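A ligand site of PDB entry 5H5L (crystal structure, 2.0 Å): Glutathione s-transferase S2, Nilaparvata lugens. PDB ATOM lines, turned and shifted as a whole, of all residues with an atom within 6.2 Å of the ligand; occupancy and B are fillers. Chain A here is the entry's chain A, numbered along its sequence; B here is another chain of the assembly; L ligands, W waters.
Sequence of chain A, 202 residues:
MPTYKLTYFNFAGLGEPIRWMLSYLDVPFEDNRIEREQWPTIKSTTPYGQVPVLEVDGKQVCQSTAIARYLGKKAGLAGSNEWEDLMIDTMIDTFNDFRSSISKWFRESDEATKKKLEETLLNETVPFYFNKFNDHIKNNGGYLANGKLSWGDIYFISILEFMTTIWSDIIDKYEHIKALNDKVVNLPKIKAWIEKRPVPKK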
ATOM      1  N   TYR A   8     -18.228 -13.666 -11.525  1.00  0.00           N
ATOM      2  CA  TYR A   8     -18.137 -13.135 -10.181  1.00  0.00           C
ATOM      3  C   TYR A   8     -16.662 -12.803  -9.925  1.00  0.00           C
ATOM      4  O   TYR A   8     -15.786 -13.092 -10.741  1.00  0.00           O
ATOM      5  CB  TYR A   8     -18.659 -14.132  -9.128  1.00  0.00           C
ATOM      6  CG  TYR A   8     -18.774 -13.545  -7.739  1.00  0.00           C
ATOM      7  CD1 TYR A   8     -19.699 -12.535  -7.457  1.00  0.00           C
ATOM      8  CD2 TYR A   8     -17.938 -13.975  -6.718  1.00  0.00           C
ATOM      9  CE1 TYR A   8     -19.796 -11.977  -6.171  1.00  0.00           C
ATOM     10  CE2 TYR A   8     -18.031 -13.431  -5.434  1.00  0.00           C
ATOM     11  CZ  TYR A   8     -18.967 -12.434  -5.190  1.00  0.00           C
ATOM     12  OH  TYR A   8     -19.090 -11.893  -3.948  1.00  0.00           O
ATOM     13  N   PHE A   9     -16.390 -12.217  -8.765  1.00  0.00           N
ATOM     14  CA  PHE A   9     -15.020 -11.944  -8.376  1.00  0.00           C
ATOM     15  C   PHE A   9     -14.242 -13.232  -8.104  1.00  0.00           C
ATOM     16  O   PHE A   9     -14.817 -14.323  -7.959  1.00  0.00           O
ATOM     17  CB  PHE A   9     -15.024 -11.035  -7.155  1.00  0.00           C
ATOM     18  CG  PHE A   9     -15.594  -9.695  -7.439  1.00  0.00           C
ATOM     19  CD1 PHE A   9     -15.014  -8.870  -8.397  1.00  0.00           C
ATOM     20  CD2 PHE A   9     -16.720  -9.258  -6.808  1.00  0.00           C
ATOM     21  CE1 PHE A   9     -15.561  -7.643  -8.669  1.00  0.00           C
ATOM     22  CE2 PHE A   9     -17.245  -8.017  -7.077  1.00  0.00           C
ATOM     23  CZ  PHE A   9     -16.675  -7.219  -8.020  1.00  0.00           C
ATOM     24  N   PHE A  11     -13.054 -14.629  -5.617  1.00  0.00           N
ATOM     25  CA  PHE A  11     -13.172 -15.247  -4.296  1.00  0.00           C
ATOM     26  C   PHE A  11     -14.540 -15.888  -4.208  1.00  0.00           C
ATOM     27  O   PHE A  11     -15.343 -15.825  -5.159  1.00  0.00           O
ATOM     28  CB  PHE A  11     -12.988 -14.233  -3.155  1.00  0.00           C
ATOM     29  CG  PHE A  11     -13.791 -12.965  -3.301  1.00  0.00           C
ATOM     30  CD1 PHE A  11     -15.056 -12.859  -2.757  1.00  0.00           C
ATOM     31  CD2 PHE A  11     -13.263 -11.868  -3.971  1.00  0.00           C
ATOM     32  CE1 PHE A  11     -15.785 -11.697  -2.899  1.00  0.00           C
ATOM     33  CE2 PHE A  11     -13.988 -10.692  -4.092  1.00  0.00           C
ATOM     34  CZ  PHE A  11     -15.232 -10.600  -3.568  1.00  0.00           C
ATOM     35  N   GLY A  13     -17.511 -15.546  -1.839  1.00  0.00           N
ATOM     36  CA  GLY A  13     -18.582 -14.559  -1.780  1.00  0.00           C
ATOM     37  C   GLY A  13     -19.944 -15.075  -2.227  1.00  0.00           C
ATOM     38  O   GLY A  13     -20.317 -16.221  -1.945  1.00  0.00           O
ATOM     39  N   LEU A  14     -20.698 -14.229  -2.925  1.00  0.00           N
ATOM     40  CA  LEU A  14     -22.023 -14.630  -3.386  1.00  0.00           C
ATOM     41  C   LEU A  14     -21.990 -15.419  -4.681  1.00  0.00           C
ATOM     42  O   LEU A  14     -23.066 -15.792  -5.169  1.00  0.00           O
ATOM     43  CB  LEU A  14     -22.941 -13.409  -3.606  1.00  0.00           C
ATOM     44  CG  LEU A  14     -23.288 -12.486  -2.450  1.00  0.00           C
ATOM     45  CD1 LEU A  14     -24.204 -11.396  -3.013  1.00  0.00           C
ATOM     46  CD2 LEU A  14     -23.963 -13.244  -1.329  1.00  0.00           C
ATOM     47  N   ARG A  36     -10.184  -7.591  -9.422  1.00  0.00           N
ATOM     48  CA  ARG A  36     -10.686  -6.262  -9.081  1.00  0.00           C
ATOM     49  C   ARG A  36     -10.238  -5.236 -10.117  1.00  0.00           C
ATOM     50  O   ARG A  36     -11.027  -4.378 -10.536  1.00  0.00           O
ATOM     51  CB  ARG A  36     -10.210  -5.882  -7.677  1.00  0.00           C
ATOM     52  CG  ARG A  36     -10.820  -4.602  -7.159  1.00  0.00           C
ATOM     53  CD  ARG A  36     -12.347  -4.683  -7.063  1.00  0.00           C
ATOM     54  NE  ARG A  36     -12.791  -5.660  -6.060  1.00  0.00           N
ATOM     55  CZ  ARG A  36     -14.054  -5.824  -5.679  1.00  0.00           C
ATOM     56  NH1 ARG A  36     -14.355  -6.730  -4.761  1.00  0.00           N
ATOM     57  NH2 ARG A  36     -15.015  -5.082  -6.216  1.00  0.00           N
ATOM     58  N   TRP A  39     -12.683  -5.078 -12.858  1.00  0.00           N
ATOM     59  CA  TRP A  39     -14.100  -4.911 -12.525  1.00  0.00           C
ATOM     60  C   TRP A  39     -14.717  -3.616 -13.059  1.00  0.00           C
ATOM     61  O   TRP A  39     -15.910  -3.630 -13.407  1.00  0.00           O
ATOM     62  CB  TRP A  39     -14.285  -5.006 -11.018  1.00  0.00           C
ATOM     63  CG  TRP A  39     -15.658  -4.647 -10.572  1.00  0.00           C
ATOM     64  CD1 TRP A  39     -16.008  -3.690  -9.671  1.00  0.00           C
ATOM     65  CD2 TRP A  39     -16.882  -5.248 -11.039  1.00  0.00           C
ATOM     66  NE1 TRP A  39     -17.379  -3.651  -9.537  1.00  0.00           N
ATOM     67  CE2 TRP A  39     -17.930  -4.602 -10.360  1.00  0.00           C
ATOM     68  CE3 TRP A  39     -17.190  -6.278 -11.931  1.00  0.00           C
ATOM     69  CZ2 TRP A  39     -19.259  -4.951 -10.552  1.00  0.00           C
ATOM     70  CZ3 TRP A  39     -18.520  -6.619 -12.144  1.00  0.00           C
ATOM     71  CH2 TRP A  39     -19.532  -5.956 -11.458  1.00  0.00           C
ATOM     72  N   LYS A  43     -18.118  -4.026 -15.108  1.00  0.00           N
ATOM     73  CA  LYS A  43     -19.315  -3.666 -14.354  1.00  0.00           C
ATOM     74  C   LYS A  43     -20.422  -3.133 -15.254  1.00  0.00           C
ATOM     75  O   LYS A  43     -21.611  -3.448 -15.060  1.00  0.00           O
ATOM     76  CB  LYS A  43     -18.937  -2.627 -13.285  1.00  0.00           C
ATOM     77  CG  LYS A  43     -20.087  -1.991 -12.505  1.00  0.00           C
ATOM     78  CD  LYS A  43     -19.538  -0.918 -11.520  1.00  0.00           C
ATOM     79  CE  LYS A  43     -20.632  -0.234 -10.696  1.00  0.00           C
ATOM     80  NZ  LYS A  43     -21.221  -1.139  -9.640  1.00  0.00           N
ATOM     81  N   GLY A  49     -25.274  -3.617 -12.682  1.00  0.00           N
ATOM     82  CA  GLY A  49     -24.059  -3.096 -12.116  1.00  0.00           C
ATOM     83  C   GLY A  49     -23.390  -3.972 -11.078  1.00  0.00           C
ATOM     84  O   GLY A  49     -22.445  -3.527 -10.434  1.00  0.00           O
ATOM     85  N   GLN A  50     -23.852  -5.205 -10.901  1.00  0.00           N
ATOM     86  CA  GLN A  50     -23.310  -6.060  -9.847  1.00  0.00           C
ATOM     87  C   GLN A  50     -23.200  -7.472 -10.363  1.00  0.00           C
ATOM     88  O   GLN A  50     -23.744  -7.830 -11.400  1.00  0.00           O
ATOM     89  CB  GLN A  50     -24.190  -6.032  -8.605  1.00  0.00           C
ATOM     90  CG  GLN A  50     -24.211  -4.688  -7.845  1.00  0.00           C
ATOM     91  CD  GLN A  50     -24.520  -4.874  -6.366  1.00  0.00           C
ATOM     92  OE1 GLN A  50     -25.621  -5.293  -6.003  1.00  0.00           O
ATOM     93  NE2 GLN A  50     -23.528  -4.608  -5.517  1.00  0.00           N
ATOM     94  N   VAL A  51     -22.400  -8.243  -9.628  1.00  0.00           N
ATOM     95  CA  VAL A  51     -22.238  -9.681  -9.832  1.00  0.00           C
ATOM     96  C   VAL A  51     -22.655 -10.371  -8.551  1.00  0.00           C
ATOM     97  O   VAL A  51     -22.645  -9.777  -7.454  1.00  0.00           O
ATOM     98  CB  VAL A  51     -20.800 -10.024 -10.259  1.00  0.00           C
ATOM     99  CG1 VAL A  51     -20.589  -9.540 -11.679  1.00  0.00           C
ATOM    100  CG2 VAL A  51     -19.725  -9.388  -9.268  1.00  0.00           C
ATOM    101  N   PRO A  52     -23.005 -11.649  -8.618  1.00  0.00           N
ATOM    102  CA  PRO A  52     -22.854 -12.588  -9.723  1.00  0.00           C
ATOM    103  C   PRO A  52     -23.854 -12.377 -10.845  1.00  0.00           C
ATOM    104  O   PRO A  52     -24.976 -11.902 -10.620  1.00  0.00           O
ATOM    105  CB  PRO A  52     -23.084 -13.936  -9.036  1.00  0.00           C
ATOM    106  CG  PRO A  52     -23.950 -13.659  -7.947  1.00  0.00           C
ATOM    107  CD  PRO A  52     -23.562 -12.307  -7.434  1.00  0.00           C
ATOM    108  N   CYS A  62     -29.156 -12.199 -13.212  1.00  0.00           N
ATOM    109  CA  CYS A  62     -28.476 -11.884 -11.969  1.00  0.00           C
ATOM    110  C   CYS A  62     -29.306 -12.333 -10.768  1.00  0.00           C
ATOM    111  O   CYS A  62     -30.355 -12.964 -10.916  1.00  0.00           O
ATOM    112  CB  CYS A  62     -28.149 -10.399 -11.892  1.00  0.00           C
ATOM    113  SG  CYS A  62     -29.577  -9.420 -11.999  1.00  0.00           S
ATOM    114  N   GLN A  63     -28.757 -12.055  -9.595  1.00  0.00           N
ATOM    115  CA  GLN A  63     -29.363 -12.255  -8.273  1.00  0.00           C
ATOM    116  C   GLN A  63     -29.092 -13.646  -7.739  1.00  0.00           C
ATOM    117  O   GLN A  63     -29.739 -14.640  -8.133  1.00  0.00           O
ATOM    118  CB  GLN A  63     -30.865 -11.980  -8.271  1.00  0.00           C
ATOM    119  CG  GLN A  63     -31.158 -10.505  -8.476  1.00  0.00           C
ATOM    120  CD  GLN A  63     -30.540  -9.644  -7.400  1.00  0.00           C
ATOM    121  OE1 GLN A  63     -30.222 -10.115  -6.304  1.00  0.00           O
ATOM    122  NE2 GLN A  63     -30.334  -8.372  -7.706  1.00  0.00           N
ATOM    123  N   SER A  64     -28.172 -13.708  -6.769  1.00  0.00           N
ATOM    124  CA  SER A  64     -27.660 -14.987  -6.313  1.00  0.00           C
ATOM    125  C   SER A  64     -28.781 -15.856  -5.731  1.00  0.00           C
ATOM    126  O   SER A  64     -28.773 -17.066  -5.921  1.00  0.00           O
ATOM    127  CB  SER A  64     -26.539 -14.777  -5.288  1.00  0.00           C
ATOM    128  OG  SER A  64     -27.017 -14.230  -4.063  1.00  0.00           O
ATOM    129  N   THR A  65     -29.727 -15.271  -4.974  1.00  0.00           N
ATOM    130  CA  THR A  65     -30.758 -16.103  -4.372  1.00  0.00           C
ATOM    131  C   THR A  65     -31.687 -16.668  -5.438  1.00  0.00           C
ATOM    132  O   THR A  65     -32.023 -17.856  -5.414  1.00  0.00           O
ATOM    133  CB  THR A  65     -31.543 -15.297  -3.331  1.00  0.00           C
ATOM    134  OG1 THR A  65     -30.652 -14.856  -2.305  1.00  0.00           O
ATOM    135  CG2 THR A  65     -32.617 -16.149  -2.714  1.00  0.00           C
ATOM    136  N   ARG A  99     -27.156 -11.053   6.344  1.00  0.00           N
ATOM    137  CA  ARG A  99     -26.050 -10.700   5.446  1.00  0.00           C
ATOM    138  C   ARG A  99     -25.963  -9.210   5.196  1.00  0.00           C
ATOM    139  O   ARG A  99     -24.874  -8.673   4.945  1.00  0.00           O
ATOM    140  CB  ARG A  99     -26.228 -11.363   4.070  1.00  0.00           C
ATOM    141  CG  ARG A  99     -25.690 -12.700   3.907  1.00  0.00           C
ATOM    142  CD  ARG A  99     -25.228 -12.891   2.478  1.00  0.00           C
ATOM    143  NE  ARG A  99     -26.299 -12.847   1.488  1.00  0.00           N
ATOM    144  CZ  ARG A  99     -26.475 -11.890   0.576  1.00  0.00           C
ATOM    145  NH1 ARG A  99     -25.653 -10.843   0.511  1.00  0.00           N
ATOM    146  NH2 ARG A  99     -27.482 -11.991  -0.278  1.00  0.00           N
ATOM    147  N   SER A 103     -22.784  -6.650   4.788  1.00  0.00           N
ATOM    148  CA  SER A 103     -22.396  -5.919   3.591  1.00  0.00           C
ATOM    149  C   SER A 103     -21.920  -4.508   3.922  1.00  0.00           C
ATOM    150  O   SER A 103     -21.088  -3.957   3.222  1.00  0.00           O
ATOM    151  CB  SER A 103     -23.564  -5.849   2.595  1.00  0.00           C
ATOM    152  OG  SER A 103     -23.686  -7.073   1.846  1.00  0.00           O
ATOM    153  N   ARG A 107     -18.151  -2.536   3.176  1.00  0.00           N
ATOM    154  CA  ARG A 107     -18.129  -1.226   2.512  1.00  0.00           C
ATOM    155  C   ARG A 107     -17.784  -0.116   3.509  1.00  0.00           C
ATOM    156  O   ARG A 107     -16.682   0.436   3.498  1.00  0.00           O
ATOM    157  CB  ARG A 107     -19.480  -0.934   1.851  1.00  0.00           C
ATOM    158  CG  ARG A 107     -19.924  -1.922   0.753  1.00  0.00           C
ATOM    159  CD  ARG A 107     -21.455  -1.929   0.562  1.00  0.00           C
ATOM    160  NE  ARG A 107     -21.860  -1.493  -0.779  1.00  0.00           N
ATOM    161  CZ  ARG A 107     -22.448  -2.251  -1.705  1.00  0.00           C
ATOM    162  NH1 ARG A 107     -22.740  -3.538  -1.475  1.00  0.00           N
ATOM    163  NH2 ARG A 107     -22.767  -1.726  -2.886  1.00  0.00           N
ATOM    164  N   TYR A 155     -26.775 -22.687  -0.126  1.00  0.00           N
ATOM    165  CA  TYR A 155     -26.575 -21.244  -0.130  1.00  0.00           C
ATOM    166  C   TYR A 155     -26.027 -20.777   1.205  1.00  0.00           C
ATOM    167  O   TYR A 155     -25.019 -20.074   1.261  1.00  0.00           O
ATOM    168  CB  TYR A 155     -27.927 -20.587  -0.416  1.00  0.00           C
ATOM    169  CG  TYR A 155     -27.884 -19.105  -0.703  1.00  0.00           C
ATOM    170  CD1 TYR A 155     -27.908 -18.197   0.334  1.00  0.00           C
ATOM    171  CD2 TYR A 155     -27.821 -18.633  -1.982  1.00  0.00           C
ATOM    172  CE1 TYR A 155     -27.877 -16.795   0.072  1.00  0.00           C
ATOM    173  CE2 TYR A 155     -27.778 -17.271  -2.248  1.00  0.00           C
ATOM    174  CZ  TYR A 155     -27.815 -16.359  -1.218  1.00  0.00           C
ATOM    175  OH  TYR A 155     -27.787 -15.019  -1.457  1.00  0.00           O
ATOM    176  N   ASP B  93     -35.807  -9.520  -6.688  1.00  0.00           N
ATOM    177  CA  ASP B  93     -34.594  -9.377  -5.899  1.00  0.00           C
ATOM    178  C   ASP B  93     -33.866  -8.092  -6.291  1.00  0.00           C
ATOM    179  O   ASP B  93     -33.315  -7.387  -5.447  1.00  0.00           O
ATOM    180  CB  ASP B  93     -33.677 -10.593  -6.083  1.00  0.00           C
ATOM    181  CG  ASP B  93     -34.059 -11.796  -5.148  1.00  0.00           C
ATOM    182  OD1 ASP B  93     -35.024 -11.697  -4.374  1.00  0.00           O
ATOM    183  OD2 ASP B  93     -33.358 -12.820  -5.198  1.00  0.00           O
ATOM    184  N   ASP B  97     -32.954  -4.868  -3.981  1.00  0.00           N
ATOM    185  CA  ASP B  97     -31.673  -4.178  -3.919  1.00  0.00           C
ATOM    186  C   ASP B  97     -31.889  -2.682  -4.046  1.00  0.00           C
ATOM    187  O   ASP B  97     -31.309  -1.894  -3.287  1.00  0.00           O
ATOM    188  CB  ASP B  97     -30.756  -4.635  -5.050  1.00  0.00           C
ATOM    189  CG  ASP B  97     -30.113  -5.973  -4.802  1.00  0.00           C
ATOM    190  OD1 ASP B  97     -30.118  -6.452  -3.651  1.00  0.00           O
ATOM    191  OD2 ASP B  97     -29.603  -6.551  -5.794  1.00  0.00           O
HETATM  192  N1  LIG L   1     -28.734  -9.024  -4.291  1.00  0.00           N
HETATM  193  C1  LIG L   1     -27.553  -9.250  -5.102  1.00  0.00           C
HETATM  194  C2  LIG L   1     -27.244 -10.745  -5.212  1.00  0.00           C
HETATM  195  O1  LIG L   1     -26.673 -11.254  -6.215  1.00  0.00           O
HETATM  196  O2  LIG L   1     -27.565 -11.444  -4.212  1.00  0.00           O
HETATM  197  C3  LIG L   1     -26.335  -8.629  -4.356  1.00  0.00           C
HETATM  198  C4  LIG L   1     -25.176  -8.605  -5.350  1.00  0.00           C
HETATM  199  C5  LIG L   1     -24.005  -7.791  -4.735  1.00  0.00           C
HETATM  200  O3  LIG L   1     -24.110  -7.190  -3.734  1.00  0.00           O
HETATM  201  N2  LIG L   1     -22.777  -7.875  -5.510  1.00  0.00           N
HETATM  202  C6  LIG L   1     -21.556  -7.216  -5.106  1.00  0.00           C
HETATM  203  C7  LIG L   1     -20.986  -6.415  -6.283  1.00  0.00           C
HETATM  204  O4  LIG L   1     -21.203  -6.716  -7.409  1.00  0.00           O
HETATM  205  C8  LIG L   1     -20.525  -8.307  -4.852  1.00  0.00           C
HETATM  206  S1  LIG L   1     -21.020  -9.535  -3.629  1.00  0.00           S
HETATM  207  N3  LIG L   1     -20.112  -5.307  -5.941  1.00  0.00           N
HETATM  208  C9  LIG L   1     -19.443  -4.539  -6.964  1.00  0.00           C
HETATM  209  C10 LIG L   1     -20.181  -3.234  -7.219  1.00  0.00           C
HETATM  210  O5  LIG L   1     -19.630  -2.429  -7.995  1.00  0.00           O
HETATM  211  O6  LIG L   1     -21.283  -3.003  -6.660  1.00  0.00           O
HETATM  212  O   HOH W   1     -30.712 -12.505  -4.768  1.00  0.00           O
HETATM  213  O   HOH W   2     -26.428 -10.529  -8.829  1.00  0.00           O
HETATM  214  O   HOH W   3     -24.954  -8.346  -0.793  1.00  0.00           O
HETATM  215  O   HOH W   4     -29.319 -12.080  -2.499  1.00  0.00           O
HETATM  216  O   HOH W   5     -27.948  -9.238  -1.491  1.00  0.00           O
HETATM  217  O   HOH W   6     -23.300  -1.042  -7.068  1.00  0.00           O
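O of Val 51 lies within hydrogen-bond range of N2 of the ligand (2.7 Å). O5 of the ligand is in salt-bridge range of NZ of Lys 43, 2.6 Å away. NE1 of Trp 39 lies within hydrogen-bond range of O5 of the ligand (3.0 Å). O4 of the ligand sits at hydrogen-bond distance from N of Val 51, at 2.9 Å. O2 of the ligand lies within salt-bridge range of NH2 of Arg 99. S1 of the ligand lies close to OH of Tyr 8 (3.1 Å). OD1 of Asp 97 of chain B is in salt-bridge range of N1 of the ligand, 3.0 Å away. An oxygen (O1) of the ligand is in hydrogen-bond range of the backbone NH (N) of Ser 64, at 2.9 Å. The side-chain hydroxyl (OG) of Ser 64 lies within hydrogen-bond range of an oxygen (O2) of the ligand (2.8 Å). The side-chain amide oxygen (OE1) of Gln 63 sits at hydrogen-bond distance from a nitrogen (N1) of the ligand, at 2.7 Å. The side-chain amide nitrogen (NE2) of Gln 50 sits at hydrogen-bond distance from an oxygen (O6) of the ligand, at 3.0 Å.
The side-chain amino group (NZ) of Lys 43 lies within hydrogen-bond range of the backbone carbonyl oxygen (O) of Gly 49 (2.8 Å). The backbone NH (N) of Leu 14 lies within hydrogen-bond range of the side-chain hydroxyl (OH) of Tyr 8. NE2 of Gln 63 is in hydrogen-bond range of OD2 of Asp 97 of chain B (2.7 Å). The side-chain hydroxyl (OH) of Tyr 155 is in hydrogen-bond range of the guanidinium group (NH2) of Arg 99, at 3.3 Å. The side-chain hydroxyl (OG) of Ser 64 is in hydrogen-bond range of the side-chain hydroxyl (OH) of Tyr 155.
CE2 of Phe 9 touches C8 of the ligand (3.97 Å). CD1 of Leu 14 touches O2 of the ligand, 3.6 Å away. Gly 49 touches the ligand. Pro 52 touches the ligand. Hydrophobic or aromatic side chains within 4 Å of the ligand: Tyr 8, Phe 9, Leu 14, Trp 39, Val 51 and Pro 52. Of the 22 residues printed, 13 come within 4 Å of the ligand. Along chain A the residues within 4 Å of the ligand span positions 8 to 99. The nearest printed residue that does not touch the ligand is Arg 107 (4.3 Å).
Water W4 lies within hydrogen-bond range of O2 of the ligand (2.5 Å), NH2 of Arg 99 (2.9 Å), OG1 of Thr 65 (3.1 Å) and OH of Tyr 155 (3.5 Å). Water W2 lies within hydrogen-bond range of O of Pro 52 (2.7 Å), O1 of the ligand (2.7 Å) and N of Gln 63 (2.9 Å). Water W6 bridges an oxygen (O6) of the ligand (2.8 Å) and the side-chain amino group of Lys 43 (3.3 Å). Water W5 bridges a nitrogen (N1) of the ligand (2.9 Å) and the guanidinium group of Arg 99 (3.0 Å). Water W3 lies within hydrogen-bond range of the guanidinium group of Arg 99 (2.9 Å), the side-chain hydroxyl of Ser 103 (3.2 Å) and an oxygen (O3) of the ligand (3.3 Å). Water W1 lies within hydrogen-bond range of the side-chain carboxylate of Asp 93 of chain B, the side-chain amide oxygen of Gln 63, the backbone NH of Thr 65, an oxygen (O2) of the ligand and the backbone NH of Ser 64.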
